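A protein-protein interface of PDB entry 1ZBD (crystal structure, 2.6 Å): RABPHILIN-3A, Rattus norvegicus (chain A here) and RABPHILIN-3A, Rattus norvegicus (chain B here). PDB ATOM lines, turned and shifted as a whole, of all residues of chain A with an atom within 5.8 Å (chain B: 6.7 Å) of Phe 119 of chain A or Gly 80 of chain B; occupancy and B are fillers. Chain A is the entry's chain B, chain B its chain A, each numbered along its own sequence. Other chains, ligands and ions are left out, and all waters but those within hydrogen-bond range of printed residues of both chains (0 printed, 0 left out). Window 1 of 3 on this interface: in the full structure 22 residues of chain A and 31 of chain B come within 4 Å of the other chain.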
ATOM      1  N   GLY A 115     -16.424  32.101  16.131  1.00  0.00           N
ATOM      2  CA  GLY A 115     -16.794  31.219  15.041  1.00  0.00           C
ATOM      3  C   GLY A 115     -16.343  31.738  13.686  1.00  0.00           C
ATOM      4  O   GLY A 115     -16.612  31.111  12.664  1.00  0.00           O
ATOM      5  N   ALA A 116     -15.663  32.880  13.665  1.00  0.00           N
ATOM      6  CA  ALA A 116     -15.192  33.444  12.401  1.00  0.00           C
ATOM      7  C   ALA A 116     -14.176  32.533  11.741  1.00  0.00           C
ATOM      8  O   ALA A 116     -14.010  32.583  10.531  1.00  0.00           O
ATOM      9  CB  ALA A 116     -14.579  34.827  12.614  1.00  0.00           C
ATOM     10  N   TRP A 117     -13.495  31.701  12.530  1.00  0.00           N
ATOM     11  CA  TRP A 117     -12.503  30.784  11.970  1.00  0.00           C
ATOM     12  C   TRP A 117     -13.168  29.850  10.958  1.00  0.00           C
ATOM     13  O   TRP A 117     -12.529  29.364  10.028  1.00  0.00           O
ATOM     14  CB  TRP A 117     -11.847  29.936  13.071  1.00  0.00           C
ATOM     15  CG  TRP A 117     -12.791  28.950  13.715  1.00  0.00           C
ATOM     16  CD1 TRP A 117     -13.541  29.148  14.836  1.00  0.00           C
ATOM     17  CD2 TRP A 117     -13.146  27.654  13.218  1.00  0.00           C
ATOM     18  NE1 TRP A 117     -14.349  28.060  15.067  1.00  0.00           N
ATOM     19  CE2 TRP A 117     -14.130  27.129  14.089  1.00  0.00           C
ATOM     20  CE3 TRP A 117     -12.737  26.886  12.120  1.00  0.00           C
ATOM     21  CZ2 TRP A 117     -14.710  25.868  13.895  1.00  0.00           C
ATOM     22  CZ3 TRP A 117     -13.315  25.630  11.926  1.00  0.00           C
ATOM     23  CH2 TRP A 117     -14.291  25.137  12.811  1.00  0.00           C
ATOM     24  N   PHE A 118     -14.457  29.603  11.144  1.00  0.00           N
ATOM     25  CA  PHE A 118     -15.196  28.719  10.255  1.00  0.00           C
ATOM     26  C   PHE A 118     -15.548  29.381   8.933  1.00  0.00           C
ATOM     27  O   PHE A 118     -15.184  28.880   7.872  1.00  0.00           O
ATOM     28  CB  PHE A 118     -16.475  28.245  10.936  1.00  0.00           C
ATOM     29  CG  PHE A 118     -17.248  27.241  10.142  1.00  0.00           C
ATOM     30  CD1 PHE A 118     -16.710  25.988   9.865  1.00  0.00           C
ATOM     31  CD2 PHE A 118     -18.527  27.538   9.685  1.00  0.00           C
ATOM     32  CE1 PHE A 118     -17.438  25.047   9.147  1.00  0.00           C
ATOM     33  CE2 PHE A 118     -19.260  26.598   8.966  1.00  0.00           C
ATOM     34  CZ  PHE A 118     -18.716  25.355   8.698  1.00  0.00           C
ATOM     35  N   PHE A 119     -16.259  30.505   9.002  1.00  0.00           N
ATOM     36  CA  PHE A 119     -16.674  31.233   7.805  1.00  0.00           C
ATOM     37  C   PHE A 119     -15.579  32.143   7.275  1.00  0.00           C
ATOM     38  O   PHE A 119     -15.792  32.880   6.312  1.00  0.00           O
ATOM     39  CB  PHE A 119     -17.907  32.090   8.094  1.00  0.00           C
ATOM     40  CG  PHE A 119     -18.967  31.380   8.873  1.00  0.00           C
ATOM     41  CD1 PHE A 119     -18.910  31.334  10.265  1.00  0.00           C
ATOM     42  CD2 PHE A 119     -20.008  30.727   8.219  1.00  0.00           C
ATOM     43  CE1 PHE A 119     -19.878  30.645  10.999  1.00  0.00           C
ATOM     44  CE2 PHE A 119     -20.980  30.036   8.940  1.00  0.00           C
ATOM     45  CZ  PHE A 119     -20.915  29.994  10.334  1.00  0.00           C
ATOM     46  N   LYS A 120     -14.408  32.095   7.902  1.00  0.00           N
ATOM     47  CA  LYS A 120     -13.297  32.946   7.493  1.00  0.00           C
ATOM     48  C   LYS A 120     -13.754  34.411   7.548  1.00  0.00           C
ATOM     49  O   LYS A 120     -13.223  35.272   6.843  1.00  0.00           O
ATOM     50  CB  LYS A 120     -12.846  32.584   6.077  1.00  0.00           C
ATOM     51  CG  LYS A 120     -12.462  31.127   5.901  1.00  0.00           C
ATOM     52  CD  LYS A 120     -11.908  30.887   4.505  1.00  0.00           C
ATOM     53  CE  LYS A 120     -11.620  29.414   4.255  1.00  0.00           C
ATOM     54  NZ  LYS A 120     -12.861  28.587   4.274  1.00  0.00           N
ATOM     55  N   GLY A 121     -14.746  34.676   8.395  1.00  0.00           N
ATOM     56  CA  GLY A 121     -15.281  36.017   8.548  1.00  0.00           C
ATOM     57  C   GLY A 121     -16.610  35.980   9.283  1.00  0.00           C
ATOM     58  O   GLY A 121     -17.056  34.916   9.707  1.00  0.00           O
ATOM     59  N   PHE A 122     -17.249  37.136   9.435  1.00  0.00           N
ATOM     60  CA  PHE A 122     -18.534  37.209  10.126  1.00  0.00           C
ATOM     61  C   PHE A 122     -19.697  37.270   9.133  1.00  0.00           C
ATOM     62  O   PHE A 122     -19.903  38.287   8.467  1.00  0.00           O
ATOM     63  CB  PHE A 122     -18.580  38.436  11.049  1.00  0.00           C
ATOM     64  CG  PHE A 122     -17.511  38.443  12.112  1.00  0.00           C
ATOM     65  CD1 PHE A 122     -16.177  38.683  11.782  1.00  0.00           C
ATOM     66  CD2 PHE A 122     -17.837  38.199  13.444  1.00  0.00           C
ATOM     67  CE1 PHE A 122     -15.181  38.680  12.766  1.00  0.00           C
ATOM     68  CE2 PHE A 122     -16.848  38.194  14.436  1.00  0.00           C
ATOM     69  CZ  PHE A 122     -15.519  38.434  14.096  1.00  0.00           C
ATOM     70  N   PRO A 123     -20.466  36.173   9.014  1.00  0.00           N
ATOM     71  CA  PRO A 123     -21.615  36.094   8.102  1.00  0.00           C
ATOM     72  C   PRO A 123     -22.897  36.685   8.703  1.00  0.00           C
ATOM     73  O   PRO A 123     -22.933  37.056   9.880  1.00  0.00           O
ATOM     74  CB  PRO A 123     -21.734  34.598   7.842  1.00  0.00           C
ATOM     75  CG  PRO A 123     -21.383  34.025   9.178  1.00  0.00           C
ATOM     76  CD  PRO A 123     -20.167  34.846   9.588  1.00  0.00           C
ATOM     77  N   PHE B   9     -21.219  25.901  19.031  1.00  0.00           N
ATOM     78  CA  PHE B   9     -21.287  25.114  17.801  1.00  0.00           C
ATOM     79  C   PHE B   9     -22.726  24.870  17.404  1.00  0.00           C
ATOM     80  O   PHE B   9     -23.545  24.433  18.218  1.00  0.00           O
ATOM     81  CB  PHE B   9     -20.581  23.760  17.974  1.00  0.00           C
ATOM     82  CG  PHE B   9     -19.094  23.869  18.173  1.00  0.00           C
ATOM     83  CD1 PHE B   9     -18.445  25.094  18.035  1.00  0.00           C
ATOM     84  CD2 PHE B   9     -18.343  22.754  18.510  1.00  0.00           C
ATOM     85  CE1 PHE B   9     -17.070  25.200  18.235  1.00  0.00           C
ATOM     86  CE2 PHE B   9     -16.968  22.852  18.709  1.00  0.00           C
ATOM     87  CZ  PHE B   9     -16.330  24.081  18.572  1.00  0.00           C
ATOM     88  N   LYS B  10     -23.032  25.169  16.148  1.00  0.00           N
ATOM     89  CA  LYS B  10     -24.366  24.960  15.613  1.00  0.00           C
ATOM     90  C   LYS B  10     -24.319  23.593  14.928  1.00  0.00           C
ATOM     91  O   LYS B  10     -23.433  23.328  14.113  1.00  0.00           O
ATOM     92  CB  LYS B  10     -24.702  26.065  14.610  1.00  0.00           C
ATOM     93  CG  LYS B  10     -26.107  25.998  14.040  1.00  0.00           C
ATOM     94  CD  LYS B  10     -26.397  27.217  13.168  1.00  0.00           C
ATOM     95  CE  LYS B  10     -27.800  27.168  12.569  1.00  0.00           C
ATOM     96  NZ  LYS B  10     -28.117  28.413  11.805  1.00  0.00           N
ATOM     97  N   ILE B  11     -25.249  22.716  15.290  1.00  0.00           N
ATOM     98  CA  ILE B  11     -25.300  21.370  14.727  1.00  0.00           C
ATOM     99  C   ILE B  11     -26.681  21.045  14.182  1.00  0.00           C
ATOM    100  O   ILE B  11     -27.693  21.329  14.826  1.00  0.00           O
ATOM    101  CB  ILE B  11     -24.938  20.308  15.791  1.00  0.00           C
ATOM    102  CG1 ILE B  11     -23.510  20.531  16.284  1.00  0.00           C
ATOM    103  CG2 ILE B  11     -25.094  18.909  15.213  1.00  0.00           C
ATOM    104  CD1 ILE B  11     -23.038  19.490  17.280  1.00  0.00           C
ATOM    105  N   LEU B  12     -26.715  20.457  12.989  1.00  0.00           N
ATOM    106  CA  LEU B  12     -27.969  20.070  12.349  1.00  0.00           C
ATOM    107  C   LEU B  12     -28.060  18.548  12.198  1.00  0.00           C
ATOM    108  O   LEU B  12     -27.072  17.882  11.874  1.00  0.00           O
ATOM    109  CB  LEU B  12     -28.079  20.708  10.968  1.00  0.00           C
ATOM    110  CG  LEU B  12     -28.999  21.912  10.824  1.00  0.00           C
ATOM    111  CD1 LEU B  12     -28.443  23.089  11.599  1.00  0.00           C
ATOM    112  CD2 LEU B  12     -29.130  22.252   9.356  1.00  0.00           C
ATOM    113  N   ALA B  76     -32.298  26.197   4.441  1.00  0.00           N
ATOM    114  CA  ALA B  76     -31.922  27.581   4.680  1.00  0.00           C
ATOM    115  C   ALA B  76     -31.039  27.695   5.924  1.00  0.00           C
ATOM    116  O   ALA B  76     -30.264  28.642   6.051  1.00  0.00           O
ATOM    117  CB  ALA B  76     -33.171  28.438   4.833  1.00  0.00           C
ATOM    118  N   TYR B  77     -31.149  26.729   6.835  1.00  0.00           N
ATOM    119  CA  TYR B  77     -30.346  26.758   8.052  1.00  0.00           C
ATOM    120  C   TYR B  77     -29.029  26.002   7.950  1.00  0.00           C
ATOM    121  O   TYR B  77     -28.278  25.950   8.916  1.00  0.00           O
ATOM    122  CB  TYR B  77     -31.131  26.203   9.241  1.00  0.00           C
ATOM    123  CG  TYR B  77     -32.279  27.073   9.687  1.00  0.00           C
ATOM    124  CD1 TYR B  77     -33.530  26.983   9.077  1.00  0.00           C
ATOM    125  CD2 TYR B  77     -32.108  28.007  10.709  1.00  0.00           C
ATOM    126  CE1 TYR B  77     -34.584  27.808   9.476  1.00  0.00           C
ATOM    127  CE2 TYR B  77     -33.151  28.836  11.114  1.00  0.00           C
ATOM    128  CZ  TYR B  77     -34.383  28.732  10.493  1.00  0.00           C
ATOM    129  OH  TYR B  77     -35.403  29.564  10.882  1.00  0.00           O
ATOM    130  N   TYR B  78     -28.741  25.420   6.791  1.00  0.00           N
ATOM    131  CA  TYR B  78     -27.497  24.670   6.621  1.00  0.00           C
ATOM    132  C   TYR B  78     -26.264  25.551   6.651  1.00  0.00           C
ATOM    133  O   TYR B  78     -25.285  25.224   7.314  1.00  0.00           O
ATOM    134  CB  TYR B  78     -27.488  23.911   5.294  1.00  0.00           C
ATOM    135  CG  TYR B  78     -28.256  22.609   5.269  1.00  0.00           C
ATOM    136  CD1 TYR B  78     -29.465  22.468   5.944  1.00  0.00           C
ATOM    137  CD2 TYR B  78     -27.823  21.550   4.470  1.00  0.00           C
ATOM    138  CE1 TYR B  78     -30.227  21.309   5.814  1.00  0.00           C
ATOM    139  CE2 TYR B  78     -28.576  20.394   4.332  1.00  0.00           C
ATOM    140  CZ  TYR B  78     -29.779  20.277   5.001  1.00  0.00           C
ATOM    141  OH  TYR B  78     -30.543  19.140   4.829  1.00  0.00           O
ATOM    142  N   ARG B  79     -26.308  26.667   5.929  1.00  0.00           N
ATOM    143  CA  ARG B  79     -25.152  27.554   5.855  1.00  0.00           C
ATOM    144  C   ARG B  79     -24.558  28.019   7.180  1.00  0.00           C
ATOM    145  O   ARG B  79     -23.436  28.519   7.207  1.00  0.00           O
ATOM    146  CB  ARG B  79     -25.449  28.761   4.955  1.00  0.00           C
ATOM    147  CG  ARG B  79     -26.752  29.491   5.202  1.00  0.00           C
ATOM    148  CD  ARG B  79     -26.828  30.734   4.308  1.00  0.00           C
ATOM    149  NE  ARG B  79     -28.133  31.389   4.365  1.00  0.00           N
ATOM    150  CZ  ARG B  79     -29.250  30.887   3.841  1.00  0.00           C
ATOM    151  NH1 ARG B  79     -29.232  29.716   3.214  1.00  0.00           N
ATOM    152  NH2 ARG B  79     -30.391  31.556   3.950  1.00  0.00           N
ATOM    153  N   GLY B  80     -25.283  27.848   8.279  1.00  0.00           N
ATOM    154  CA  GLY B  80     -24.735  28.259   9.559  1.00  0.00           C
ATOM    155  C   GLY B  80     -24.120  27.113  10.347  1.00  0.00           C
ATOM    156  O   GLY B  80     -23.407  27.331  11.327  1.00  0.00           O
ATOM    157  N   ALA B  81     -24.385  25.887   9.905  1.00  0.00           N
ATOM    158  CA  ALA B  81     -23.904  24.681  10.573  1.00  0.00           C
ATOM    159  C   ALA B  81     -22.412  24.407  10.514  1.00  0.00           C
ATOM    160  O   ALA B  81     -21.766  24.607   9.493  1.00  0.00           O
ATOM    161  CB  ALA B  81     -24.643  23.481  10.032  1.00  0.00           C
ATOM    162  N   MET B  82     -21.880  23.920  11.630  1.00  0.00           N
ATOM    163  CA  MET B  82     -20.473  23.569  11.741  1.00  0.00           C
ATOM    164  C   MET B  82     -20.341  22.053  11.662  1.00  0.00           C
ATOM    165  O   MET B  82     -19.275  21.524  11.345  1.00  0.00           O
ATOM    166  CB  MET B  82     -19.898  24.076  13.071  1.00  0.00           C
ATOM    167  CG  MET B  82     -19.337  25.487  12.988  1.00  0.00           C
ATOM    168  SD  MET B  82     -18.954  26.240  14.573  1.00  0.00           S
ATOM    169  CE  MET B  82     -20.345  27.368  14.629  1.00  0.00           C
ATOM    170  N   GLY B  83     -21.435  21.357  11.953  1.00  0.00           N
ATOM    171  CA  GLY B  83     -21.411  19.910  11.905  1.00  0.00           C
ATOM    172  C   GLY B  83     -22.769  19.311  11.615  1.00  0.00           C
ATOM    173  O   GLY B  83     -23.803  19.871  11.999  1.00  0.00           O
ATOM    174  N   TYR B 109     -25.863  23.412   0.146  1.00  0.00           N
ATOM    175  CA  TYR B 109     -26.241  24.471   1.071  1.00  0.00           C
ATOM    176  C   TYR B 109     -25.342  24.752   2.273  1.00  0.00           C
ATOM    177  O   TYR B 109     -25.707  25.558   3.124  1.00  0.00           O
ATOM    178  CB  TYR B 109     -27.656  24.217   1.590  1.00  0.00           C
ATOM    179  CG  TYR B 109     -28.707  24.298   0.523  1.00  0.00           C
ATOM    180  CD1 TYR B 109     -29.130  25.535   0.034  1.00  0.00           C
ATOM    181  CD2 TYR B 109     -29.258  23.141  -0.030  1.00  0.00           C
ATOM    182  CE1 TYR B 109     -30.075  25.621  -0.986  1.00  0.00           C
ATOM    183  CE2 TYR B 109     -30.206  23.215  -1.048  1.00  0.00           C
ATOM    184  CZ  TYR B 109     -30.608  24.457  -1.522  1.00  0.00           C
ATOM    185  OH  TYR B 109     -31.533  24.539  -2.534  1.00  0.00           O
ATOM    186  N   SER B 110     -24.178  24.122   2.365  1.00  0.00           N
ATOM    187  CA  SER B 110     -23.327  24.372   3.523  1.00  0.00           C
ATOM    188  C   SER B 110     -21.916  24.753   3.148  1.00  0.00           C
ATOM    189  O   SER B 110     -21.488  24.564   2.010  1.00  0.00           O
ATOM    190  CB  SER B 110     -23.254  23.136   4.417  1.00  0.00           C
ATOM    191  OG  SER B 110     -22.231  22.260   3.958  1.00  0.00           O
ATOM    192  N   TRP B 111     -21.183  25.271   4.129  1.00  0.00           N
ATOM    193  CA  TRP B 111     -19.804  25.663   3.912  1.00  0.00           C
ATOM    194  C   TRP B 111     -18.909  24.440   3.808  1.00  0.00           C
ATOM    195  O   TRP B 111     -19.356  23.309   4.003  1.00  0.00           O
ATOM    196  CB  TRP B 111     -19.340  26.600   5.025  1.00  0.00           C
ATOM    197  CG  TRP B 111     -19.251  27.998   4.539  1.00  0.00           C
ATOM    198  CD1 TRP B 111     -18.182  28.584   3.921  1.00  0.00           C
ATOM    199  CD2 TRP B 111     -20.307  28.957   4.510  1.00  0.00           C
ATOM    200  NE1 TRP B 111     -18.512  29.851   3.503  1.00  0.00           N
ATOM    201  CE2 TRP B 111     -19.812  30.106   3.850  1.00  0.00           C
ATOM    202  CE3 TRP B 111     -21.627  28.960   4.971  1.00  0.00           C
ATOM    203  CZ2 TRP B 111     -20.594  31.246   3.641  1.00  0.00           C
ATOM    204  CZ3 TRP B 111     -22.405  30.096   4.763  1.00  0.00           C
ATOM    205  CH2 TRP B 111     -21.884  31.223   4.103  1.00  0.00           C
ATOM    206  N   ASN B 113     -15.811  23.579   5.594  1.00  0.00           N
ATOM    207  CA  ASN B 113     -15.302  22.932   6.796  1.00  0.00           C
ATOM    208  C   ASN B 113     -16.351  22.070   7.494  1.00  0.00           C
ATOM    209  O   ASN B 113     -16.016  21.287   8.378  1.00  0.00           O
ATOM    210  CB  ASN B 113     -14.775  23.969   7.798  1.00  0.00           C
ATOM    211  CG  ASN B 113     -13.650  24.815   7.238  1.00  0.00           C
ATOM    212  OD1 ASN B 113     -13.872  25.689   6.401  1.00  0.00           O
ATOM    213  ND2 ASN B 113     -12.431  24.558   7.700  1.00  0.00           N
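The backbone carbonyl oxygen (O) of Lys 10 of chain B is in hydrogen-bond range of the backbone NH (N) of Met 82 of chain B. The backbone NH (N) of Arg 79 of chain B sits at hydrogen-bond distance from the backbone carbonyl oxygen (O) of Tyr 109 of chain B. The backbone carbonyl oxygen (O) of Ala 76 of chain B lies within hydrogen-bond range of the guanidinium group (NH1) of Arg 79 of chain B (3.2 Å).
Among the printed residues, pairs that only touch across the chains: Phe 118 of chain A with Ala 81 of chain B, Phe 118 of chain A with Met 82 of chain B, Phe 118 of chain A with Trp 111 of chain B, Phe 118 of chain A with Asn 113 of chain B, Phe 119 of chain A with Arg 79 of chain B, Phe 119 of chain A with Gly 80 of chain B and Lys 120 of chain A with Asn 113 of chain B.
Phe 119 of chain A touches just these residues of chain B: Arg 79 and Gly 80. Of chain A, only Phe 119 (3.8 Å) comes within 4 Å of Gly 80 of chain B. Of the printed residues of chain A, Ala 81 of chain B touches Phe 118. Printed residues of chain A within 4 Å of Trp 111 of chain B: Phe 118. The nearest residue of chain B that does not touch Phe 119 of chain A is Trp 111 of chain B (4.04 Å). The nearest residue of chain A that does not touch Gly 80 of chain B is Phe 118 of chain A (4.8 Å). The nearest printed residue of chain B that does not touch Lys 120 of chain A is Trp 111 of chain B (5.3 Å).
Hydrophobic or aromatic side chains of chain A within 4 Å of the printed part of chain B: Phe 118 and Phe 119. Of the 16 printed residues of chain B, 6 touch a printed residue of chain A. Along chain B the printed residues that touch a printed residue of chain A span positions 79 to 113. Among the printed residues, 7 pairs touch across the chains.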
